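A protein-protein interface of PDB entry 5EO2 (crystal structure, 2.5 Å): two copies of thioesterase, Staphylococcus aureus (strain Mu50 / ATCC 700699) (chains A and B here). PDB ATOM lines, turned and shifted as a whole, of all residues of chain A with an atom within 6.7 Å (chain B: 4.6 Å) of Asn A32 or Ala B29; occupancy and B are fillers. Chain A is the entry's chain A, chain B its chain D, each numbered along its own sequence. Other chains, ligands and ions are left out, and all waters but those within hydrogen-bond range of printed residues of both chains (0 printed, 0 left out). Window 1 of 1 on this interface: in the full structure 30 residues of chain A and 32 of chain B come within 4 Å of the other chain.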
ATOM      1  N   HIS A  27      11.937  -1.489  27.105  1.00  0.00           N
ATOM      2  CA  HIS A  27      12.515  -2.467  26.161  1.00  0.00           C
ATOM      3  C   HIS A  27      11.587  -3.688  26.016  1.00  0.00           C
ATOM      4  O   HIS A  27      10.978  -4.124  26.997  1.00  0.00           O
ATOM      5  CB  HIS A  27      13.921  -2.895  26.613  1.00  0.00           C
ATOM      6  CG  HIS A  27      14.684  -3.673  25.581  1.00  0.00           C
ATOM      7  ND1 HIS A  27      14.881  -5.038  25.657  1.00  0.00           N
ATOM      8  CD2 HIS A  27      15.303  -3.270  24.448  1.00  0.00           C
ATOM      9  CE1 HIS A  27      15.597  -5.438  24.625  1.00  0.00           C
ATOM     10  NE2 HIS A  27      15.859  -4.386  23.872  1.00  0.00           N
ATOM     11  N   ASP A  28      11.464  -4.198  24.789  1.00  0.00           N
ATOM     12  CA  ASP A  28      10.448  -5.236  24.462  1.00  0.00           C
ATOM     13  C   ASP A  28      10.528  -6.519  25.314  1.00  0.00           C
ATOM     14  O   ASP A  28       9.517  -7.013  25.793  1.00  0.00           O
ATOM     15  CB  ASP A  28      10.487  -5.599  22.967  1.00  0.00           C
ATOM     16  CG  ASP A  28      11.859  -6.107  22.502  1.00  0.00           C
ATOM     17  OD1 ASP A  28      12.802  -6.191  23.340  1.00  0.00           O
ATOM     18  OD2 ASP A  28      11.988  -6.408  21.289  1.00  0.00           O
ATOM     19  N   ALA A  29      11.736  -7.028  25.533  1.00  0.00           N
ATOM     20  CA  ALA A  29      11.917  -8.273  26.265  1.00  0.00           C
ATOM     21  C   ALA A  29      11.675  -8.110  27.768  1.00  0.00           C
ATOM     22  O   ALA A  29      11.372  -9.092  28.461  1.00  0.00           O
ATOM     23  CB  ALA A  29      13.305  -8.841  25.996  1.00  0.00           C
ATOM     24  N   ASN A  30      11.796  -6.870  28.261  1.00  0.00           N
ATOM     25  CA  ASN A  30      11.559  -6.566  29.683  1.00  0.00           C
ATOM     26  C   ASN A  30      10.088  -6.789  30.080  1.00  0.00           C
ATOM     27  O   ASN A  30       9.789  -7.166  31.225  1.00  0.00           O
ATOM     28  CB  ASN A  30      11.999  -5.135  30.030  1.00  0.00           C
ATOM     29  CG  ASN A  30      13.496  -5.009  30.213  1.00  0.00           C
ATOM     30  OD1 ASN A  30      13.961  -4.648  31.286  1.00  0.00           O
ATOM     31  ND2 ASN A  30      14.259  -5.332  29.180  1.00  0.00           N
ATOM     32  N   TYR A  31       9.189  -6.586  29.116  1.00  0.00           N
ATOM     33  CA  TYR A  31       7.790  -6.998  29.264  1.00  0.00           C
ATOM     34  C   TYR A  31       7.722  -8.488  29.591  1.00  0.00           C
ATOM     35  O   TYR A  31       7.040  -8.882  30.543  1.00  0.00           O
ATOM     36  CB  TYR A  31       6.972  -6.721  27.992  1.00  0.00           C
ATOM     37  CG  TYR A  31       6.664  -5.252  27.730  1.00  0.00           C
ATOM     38  CD1 TYR A  31       7.646  -4.386  27.210  1.00  0.00           C
ATOM     39  CD2 TYR A  31       5.404  -4.729  28.007  1.00  0.00           C
ATOM     40  CE1 TYR A  31       7.380  -3.056  26.987  1.00  0.00           C
ATOM     41  CE2 TYR A  31       5.123  -3.391  27.775  1.00  0.00           C
ATOM     42  CZ  TYR A  31       6.106  -2.559  27.262  1.00  0.00           C
ATOM     43  OH  TYR A  31       5.821  -1.233  27.026  1.00  0.00           O
ATOM     44  N   ASN A  32       8.462  -9.287  28.823  1.00  0.00           N
ATOM     45  CA  ASN A  32       8.518 -10.753  29.036  1.00  0.00           C
ATOM     46  C   ASN A  32       9.109 -11.131  30.397  1.00  0.00           C
ATOM     47  O   ASN A  32       8.610 -12.049  31.064  1.00  0.00           O
ATOM     48  CB  ASN A  32       9.291 -11.462  27.908  1.00  0.00           C
ATOM     49  CG  ASN A  32       8.713 -11.165  26.528  1.00  0.00           C
ATOM     50  OD1 ASN A  32       8.895 -10.076  25.977  1.00  0.00           O
ATOM     51  ND2 ASN A  32       7.997 -12.125  25.974  1.00  0.00           N
ATOM     52  N   ILE A  33      10.155 -10.411  30.806  1.00  0.00           N
ATOM     53  CA  ILE A  33      10.734 -10.584  32.128  1.00  0.00           C
ATOM     54  C   ILE A  33       9.662 -10.413  33.195  1.00  0.00           C
ATOM     55  O   ILE A  33       9.527 -11.257  34.089  1.00  0.00           O
ATOM     56  CB  ILE A  33      11.902  -9.603  32.391  1.00  0.00           C
ATOM     57  CG1 ILE A  33      13.124 -10.004  31.542  1.00  0.00           C
ATOM     58  CG2 ILE A  33      12.290  -9.589  33.878  1.00  0.00           C
ATOM     59  CD1 ILE A  33      14.198  -8.931  31.457  1.00  0.00           C
ATOM     60  N   ILE A  34       8.907  -9.326  33.075  1.00  0.00           N
ATOM     61  CA  ILE A  34       7.842  -8.998  34.023  1.00  0.00           C
ATOM     62  C   ILE A  34       6.733 -10.055  34.015  1.00  0.00           C
ATOM     63  O   ILE A  34       6.333 -10.520  35.092  1.00  0.00           O
ATOM     64  CB  ILE A  34       7.238  -7.599  33.728  1.00  0.00           C
ATOM     65  CG1 ILE A  34       8.274  -6.509  34.034  1.00  0.00           C
ATOM     66  CG2 ILE A  34       5.948  -7.368  34.523  1.00  0.00           C
ATOM     67  CD1 ILE A  34       7.990  -5.213  33.328  1.00  0.00           C
ATOM     68  N   PHE A  35       6.238 -10.407  32.819  1.00  0.00           N
ATOM     69  CA  PHE A  35       5.177 -11.406  32.685  1.00  0.00           C
ATOM     70  C   PHE A  35       5.568 -12.731  33.329  1.00  0.00           C
ATOM     71  O   PHE A  35       4.745 -13.332  34.037  1.00  0.00           O
ATOM     72  CB  PHE A  35       4.791 -11.640  31.206  1.00  0.00           C
ATOM     73  CG  PHE A  35       3.980 -10.519  30.600  1.00  0.00           C
ATOM     74  CD1 PHE A  35       2.774 -10.120  31.177  1.00  0.00           C
ATOM     75  CD2 PHE A  35       4.398  -9.883  29.439  1.00  0.00           C
ATOM     76  CE1 PHE A  35       2.006  -9.098  30.614  1.00  0.00           C
ATOM     77  CE2 PHE A  35       3.637  -8.859  28.869  1.00  0.00           C
ATOM     78  CZ  PHE A  35       2.439  -8.458  29.461  1.00  0.00           C
ATOM     79  N   SER A  36       6.810 -13.169  33.084  1.00  0.00           N
ATOM     80  CA  SER A  36       7.333 -14.405  33.691  1.00  0.00           C
ATOM     81  C   SER A  36       7.360 -14.295  35.209  1.00  0.00           C
ATOM     82  O   SER A  36       6.895 -15.180  35.921  1.00  0.00           O
ATOM     83  CB  SER A  36       8.741 -14.741  33.169  1.00  0.00           C
ATOM     84  OG  SER A  36       9.177 -16.021  33.628  1.00  0.00           O
ATOM     85  N   ASP A  37       7.923 -13.197  35.688  1.00  0.00           N
ATOM     86  CA  ASP A  37       8.012 -12.923  37.130  1.00  0.00           C
ATOM     87  C   ASP A  37       6.639 -13.020  37.822  1.00  0.00           C
ATOM     88  O   ASP A  37       6.515 -13.647  38.883  1.00  0.00           O
ATOM     89  CB  ASP A  37       8.636 -11.543  37.371  1.00  0.00           C
ATOM     90  CG  ASP A  37       8.543 -11.112  38.808  1.00  0.00           C
ATOM     91  OD1 ASP A  37       8.848 -11.946  39.705  1.00  0.00           O
ATOM     92  OD2 ASP A  37       8.121  -9.944  39.074  1.00  0.00           O
ATOM     93  N   GLU A  65       4.541 -19.020  24.364  1.00  0.00           N
ATOM     94  CA  GLU A  65       4.105 -17.675  24.732  1.00  0.00           C
ATOM     95  C   GLU A  65       3.975 -16.710  23.550  1.00  0.00           C
ATOM     96  O   GLU A  65       4.759 -16.741  22.610  1.00  0.00           O
ATOM     97  CB  GLU A  65       4.984 -17.087  25.857  1.00  0.00           C
ATOM     98  CG  GLU A  65       6.363 -16.656  25.423  1.00  0.00           C
ATOM     99  CD  GLU A  65       6.460 -15.185  25.048  1.00  0.00           C
ATOM    100  OE1 GLU A  65       5.537 -14.398  25.409  1.00  0.00           O
ATOM    101  OE2 GLU A  65       7.466 -14.820  24.394  1.00  0.00           O
ATOM    102  N   HIS A  66       2.951 -15.865  23.639  1.00  0.00           N
ATOM    103  CA  HIS A  66       2.630 -14.850  22.653  1.00  0.00           C
ATOM    104  C   HIS A  66       2.603 -13.508  23.387  1.00  0.00           C
ATOM    105  O   HIS A  66       2.105 -13.400  24.521  1.00  0.00           O
ATOM    106  CB  HIS A  66       1.258 -15.159  22.019  1.00  0.00           C
ATOM    107  CG  HIS A  66       1.017 -14.466  20.713  1.00  0.00           C
ATOM    108  ND1 HIS A  66      -0.221 -14.413  20.112  1.00  0.00           N
ATOM    109  CD2 HIS A  66       1.855 -13.788  19.897  1.00  0.00           C
ATOM    110  CE1 HIS A  66      -0.134 -13.732  18.984  1.00  0.00           C
ATOM    111  NE2 HIS A  66       1.116 -13.347  18.830  1.00  0.00           N
ATOM    112  N   THR A  67       3.174 -12.487  22.764  1.00  0.00           N
ATOM    113  CA  THR A  67       3.191 -11.151  23.377  1.00  0.00           C
ATOM    114  C   THR A  67       2.813 -10.092  22.348  1.00  0.00           C
ATOM    115  O   THR A  67       3.347 -10.093  21.215  1.00  0.00           O
ATOM    116  CB  THR A  67       4.563 -10.805  23.994  1.00  0.00           C
ATOM    117  OG1 THR A  67       4.970 -11.845  24.901  1.00  0.00           O
ATOM    118  CG2 THR A  67       4.502  -9.434  24.748  1.00  0.00           C
ATOM    119  N   TYR A  69       2.473  -5.814  21.977  1.00  0.00           N
ATOM    120  CA  TYR A  69       2.819  -4.512  22.554  1.00  0.00           C
ATOM    121  C   TYR A  69       1.962  -3.443  21.899  1.00  0.00           C
ATOM    122  O   TYR A  69       2.137  -3.142  20.729  1.00  0.00           O
ATOM    123  CB  TYR A  69       4.297  -4.215  22.331  1.00  0.00           C
ATOM    124  CG  TYR A  69       5.223  -5.344  22.730  1.00  0.00           C
ATOM    125  CD1 TYR A  69       5.803  -5.397  24.010  1.00  0.00           C
ATOM    126  CD2 TYR A  69       5.533  -6.368  21.811  1.00  0.00           C
ATOM    127  CE1 TYR A  69       6.659  -6.436  24.360  1.00  0.00           C
ATOM    128  CE2 TYR A  69       6.383  -7.417  22.149  1.00  0.00           C
ATOM    129  CZ  TYR A  69       6.958  -7.449  23.414  1.00  0.00           C
ATOM    130  OH  TYR A  69       7.805  -8.498  23.700  1.00  0.00           O
ATOM    131  N   ASN A 110      -0.075 -10.830  27.174  1.00  0.00           N
ATOM    132  CA  ASN A 110       0.695 -12.054  27.189  1.00  0.00           C
ATOM    133  C   ASN A 110      -0.221 -13.274  27.210  1.00  0.00           C
ATOM    134  O   ASN A 110      -1.162 -13.322  27.982  1.00  0.00           O
ATOM    135  CB  ASN A 110       1.637 -12.076  28.394  1.00  0.00           C
ATOM    136  CG  ASN A 110       2.736 -13.125  28.258  1.00  0.00           C
ATOM    137  OD1 ASN A 110       2.869 -13.995  29.116  1.00  0.00           O
ATOM    138  ND2 ASN A 110       3.521 -13.053  27.167  1.00  0.00           N
ATOM    139  N   HIS B  27      16.342 -19.559  31.997  1.00  0.00           N
ATOM    140  CA  HIS B  27      15.055 -18.911  32.323  1.00  0.00           C
ATOM    141  C   HIS B  27      14.339 -18.520  31.019  1.00  0.00           C
ATOM    142  O   HIS B  27      14.985 -18.140  30.033  1.00  0.00           O
ATOM    143  CB  HIS B  27      15.273 -17.675  33.224  1.00  0.00           C
ATOM    144  CG  HIS B  27      14.004 -17.018  33.697  1.00  0.00           C
ATOM    145  ND1 HIS B  27      13.843 -15.647  33.740  1.00  0.00           N
ATOM    146  CD2 HIS B  27      12.838 -17.546  34.141  1.00  0.00           C
ATOM    147  CE1 HIS B  27      12.638 -15.356  34.198  1.00  0.00           C
ATOM    148  NE2 HIS B  27      12.003 -16.490  34.439  1.00  0.00           N
ATOM    149  N   ASP B  28      13.022 -18.667  31.013  1.00  0.00           N
ATOM    150  CA  ASP B  28      12.229 -18.435  29.803  1.00  0.00           C
ATOM    151  C   ASP B  28      12.363 -17.031  29.163  1.00  0.00           C
ATOM    152  O   ASP B  28      12.390 -16.915  27.933  1.00  0.00           O
ATOM    153  CB  ASP B  28      10.743 -18.752  30.081  1.00  0.00           C
ATOM    154  CG  ASP B  28      10.152 -17.922  31.230  1.00  0.00           C
ATOM    155  OD1 ASP B  28      10.833 -16.993  31.759  1.00  0.00           O
ATOM    156  OD2 ASP B  28       8.999 -18.241  31.584  1.00  0.00           O
ATOM    157  N   ALA B  29      12.457 -15.994  29.994  1.00  0.00           N
ATOM    158  CA  ALA B  29      12.553 -14.624  29.504  1.00  0.00           C
ATOM    159  C   ALA B  29      13.938 -14.295  28.882  1.00  0.00           C
ATOM    160  O   ALA B  29      14.052 -13.445  27.969  1.00  0.00           O
ATOM    161  CB  ALA B  29      12.194 -13.650  30.620  1.00  0.00           C
ATOM    162  N   ASN B  30      14.986 -14.973  29.366  1.00  0.00           N
ATOM    163  CA  ASN B  30      16.344 -14.815  28.777  1.00  0.00           C
ATOM    164  C   ASN B  30      16.387 -15.164  27.282  1.00  0.00           C
ATOM    165  O   ASN B  30      17.093 -14.510  26.521  1.00  0.00           O
ATOM    166  CB  ASN B  30      17.409 -15.621  29.544  1.00  0.00           C
ATOM    167  CG  ASN B  30      17.862 -14.931  30.829  1.00  0.00           C
ATOM    168  OD1 ASN B  30      17.411 -15.279  31.918  1.00  0.00           O
ATOM    169  ND2 ASN B  30      18.790 -13.995  30.708  1.00  0.00           N
ATOM    170  N   TYR B  31      15.590 -16.149  26.862  1.00  0.00           N
ATOM    171  CA  TYR B  31      15.432 -16.452  25.434  1.00  0.00           C
ATOM    172  C   TYR B  31      14.991 -15.189  24.685  1.00  0.00           C
ATOM    173  O   TYR B  31      15.592 -14.796  23.687  1.00  0.00           O
ATOM    174  CB  TYR B  31      14.406 -17.555  25.212  1.00  0.00           C
ATOM    175  CG  TYR B  31      14.830 -18.940  25.630  1.00  0.00           C
ATOM    176  CD1 TYR B  31      14.614 -19.404  26.933  1.00  0.00           C
ATOM    177  CD2 TYR B  31      15.403 -19.815  24.711  1.00  0.00           C
ATOM    178  CE1 TYR B  31      14.956 -20.708  27.312  1.00  0.00           C
ATOM    179  CE2 TYR B  31      15.758 -21.116  25.075  1.00  0.00           C
ATOM    180  CZ  TYR B  31      15.542 -21.565  26.374  1.00  0.00           C
ATOM    181  OH  TYR B  31      15.912 -22.846  26.734  1.00  0.00           O
ATOM    182  N   ASN B  32      13.967 -14.537  25.224  1.00  0.00           N
ATOM    183  CA  ASN B  32      13.455 -13.285  24.641  1.00  0.00           C
ATOM    184  C   ASN B  32      14.509 -12.192  24.573  1.00  0.00           C
ATOM    185  O   ASN B  32      14.568 -11.454  23.580  1.00  0.00           O
ATOM    186  CB  ASN B  32      12.206 -12.781  25.396  1.00  0.00           C
ATOM    187  CG  ASN B  32      11.120 -13.834  25.470  1.00  0.00           C
ATOM    188  OD1 ASN B  32      11.213 -14.777  26.262  1.00  0.00           O
ATOM    189  ND2 ASN B  32      10.103 -13.704  24.630  1.00  0.00           N
ATOM    190  N   ILE B  33      15.336 -12.109  25.624  1.00  0.00           N
ATOM    191  CA  ILE B  33      16.456 -11.157  25.672  1.00  0.00           C
ATOM    192  C   ILE B  33      17.425 -11.424  24.515  1.00  0.00           C
ATOM    193  O   ILE B  33      17.782 -10.502  23.777  1.00  0.00           O
ATOM    194  CB  ILE B  33      17.203 -11.201  27.046  1.00  0.00           C
ATOM    195  CG1 ILE B  33      16.284 -10.669  28.167  1.00  0.00           C
ATOM    196  CG2 ILE B  33      18.527 -10.434  27.005  1.00  0.00           C
ATOM    197  CD1 ILE B  33      16.828 -10.868  29.569  1.00  0.00           C
ATOM    198  N   GLU B  65       5.020 -10.645  18.968  1.00  0.00           N
ATOM    199  CA  GLU B  65       6.002 -11.722  18.969  1.00  0.00           C
ATOM    200  C   GLU B  65       5.514 -12.997  19.657  1.00  0.00           C
ATOM    201  O   GLU B  65       4.680 -12.970  20.572  1.00  0.00           O
ATOM    202  CB  GLU B  65       7.335 -11.252  19.582  1.00  0.00           C
ATOM    203  CG  GLU B  65       7.237 -10.809  21.026  1.00  0.00           C
ATOM    204  CD  GLU B  65       7.732 -11.852  22.012  1.00  0.00           C
ATOM    205  OE1 GLU B  65       7.926 -13.043  21.637  1.00  0.00           O
ATOM    206  OE2 GLU B  65       7.962 -11.445  23.176  1.00  0.00           O
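The side-chain hydroxyl of Tyr A69 sits at hydrogen-bond distance from the side-chain carboxylate of Glu B65, 3.0 Å away. ND2 of Asn A32 lies close to ND2 of Asn B32. The backbone NH (N) of Thr A67 sits at hydrogen-bond distance from the backbone carbonyl oxygen (O) of Glu B65 (2.7 Å). The side-chain amide nitrogen (ND2) of Asn A32 lies within hydrogen-bond range of the side-chain carboxylate (OE2) of Glu B65 (2.9 Å). The side-chain amide nitrogen (ND2) of Asn B32 sits at hydrogen-bond distance from the side-chain carboxylate (OE2) of Glu A65. The side-chain hydroxyl (OG) of Ser A36 is in hydrogen-bond range of the side-chain carboxylate (OD1) of Asp B28 (2.7 Å). OG of Ser A36 sits at hydrogen-bond distance from NE2 of His B27, 3.0 Å away. The side-chain carboxylate (OE2) of Glu A65 lies close to the side-chain carboxylate (OE1) of Glu B65 (3.3 Å).
ND2 of Asn B32 is in hydrogen-bond range of OE2 of Glu B65 (3.4 Å). The backbone carbonyl oxygen (O) of Asp B28 lies close to the side-chain amide oxygen (OD1) of Asn B32. A ring nitrogen (NE2) of His B27 sits at hydrogen-bond distance from the side-chain carboxylate (OD1) of Asp B28 (3.0 Å). The backbone carbonyl oxygen of His A66 is in hydrogen-bond range of the side-chain amide nitrogen of Asn A110 (3.0 Å). OG1 of Thr A67 sits at hydrogen-bond distance from OE1 of Glu A65 (2.7 Å). The side-chain hydroxyl of Thr A67 lies within hydrogen-bond range of the side-chain amide nitrogen of Asn A110 (2.9 Å).
Ala A29 touches Asn B32 (CB to O, 3.8 Å). Ile B33 touches Ala A29 (N to CB, 3.9 Å). Asn A32 touches Ala B29. Ile A33 touches Ala B29 (CA to CB, 3.7 Å). CD1 of Ile B33 touches CD1 of Ile A33, at 3.8 Å. His A66 touches Glu B65 (CD2 to O, 3.0 Å).
Of the printed residues of chain B, Asn A32 touches Ala B29, Asn B32 and Glu B65. Printed residues of chain A within 4 Å of Ala B29: Asn A32 and Ile A33. Of the printed residues of chain A, Asn B32 touches Ala A29, Asn A32 and Glu A65. Of the printed residues of chain B, Ser A36 touches His B27 and Asp B28. Of the printed residues of chain B, Thr A67 touches Glu B65. Printed residues of chain B within 4 Å of Tyr A69: Glu B65 (3.0 Å). Asn A30 touches none of the printed residues of chain B. The nearest printed residue of chain B that does not touch His A66 is Asn B32 (7.5 Å).
Of the 16 printed residues of chain A, 8 touch a printed residue of chain B. Hydrophobic or aromatic side chains of chain A within 4 Å of the printed part of chain B: Ala A29, Ile A33, His A66 and Tyr A69. Of the 8 printed residues of chain B, 6 touch a printed residue of chain A. Hydrophobic or aromatic side chains of chain B within 4 Å of the printed part of chain A: His B27, Ala B29 and Ile B33. Among the printed residues, 14 pairs touch across the chains. Among the printed residues, no Asp or Glu carboxylate lies within 4 Å of a Lys or Arg side-chain nitrogen of the other chain.
Ala A29 touches Asn B32, and with the chains exchanged Asn A32 touches Ala B29. Ala A29 touches Ile B33, and with the chains exchanged Ile A33 touches Ala B29. Asn A32 touches Glu B65, and with the chains exchanged Glu A65 touches Asn B32. Glu A65 touches its own counterpart, Glu B65. 8 positions are printed for both chains.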
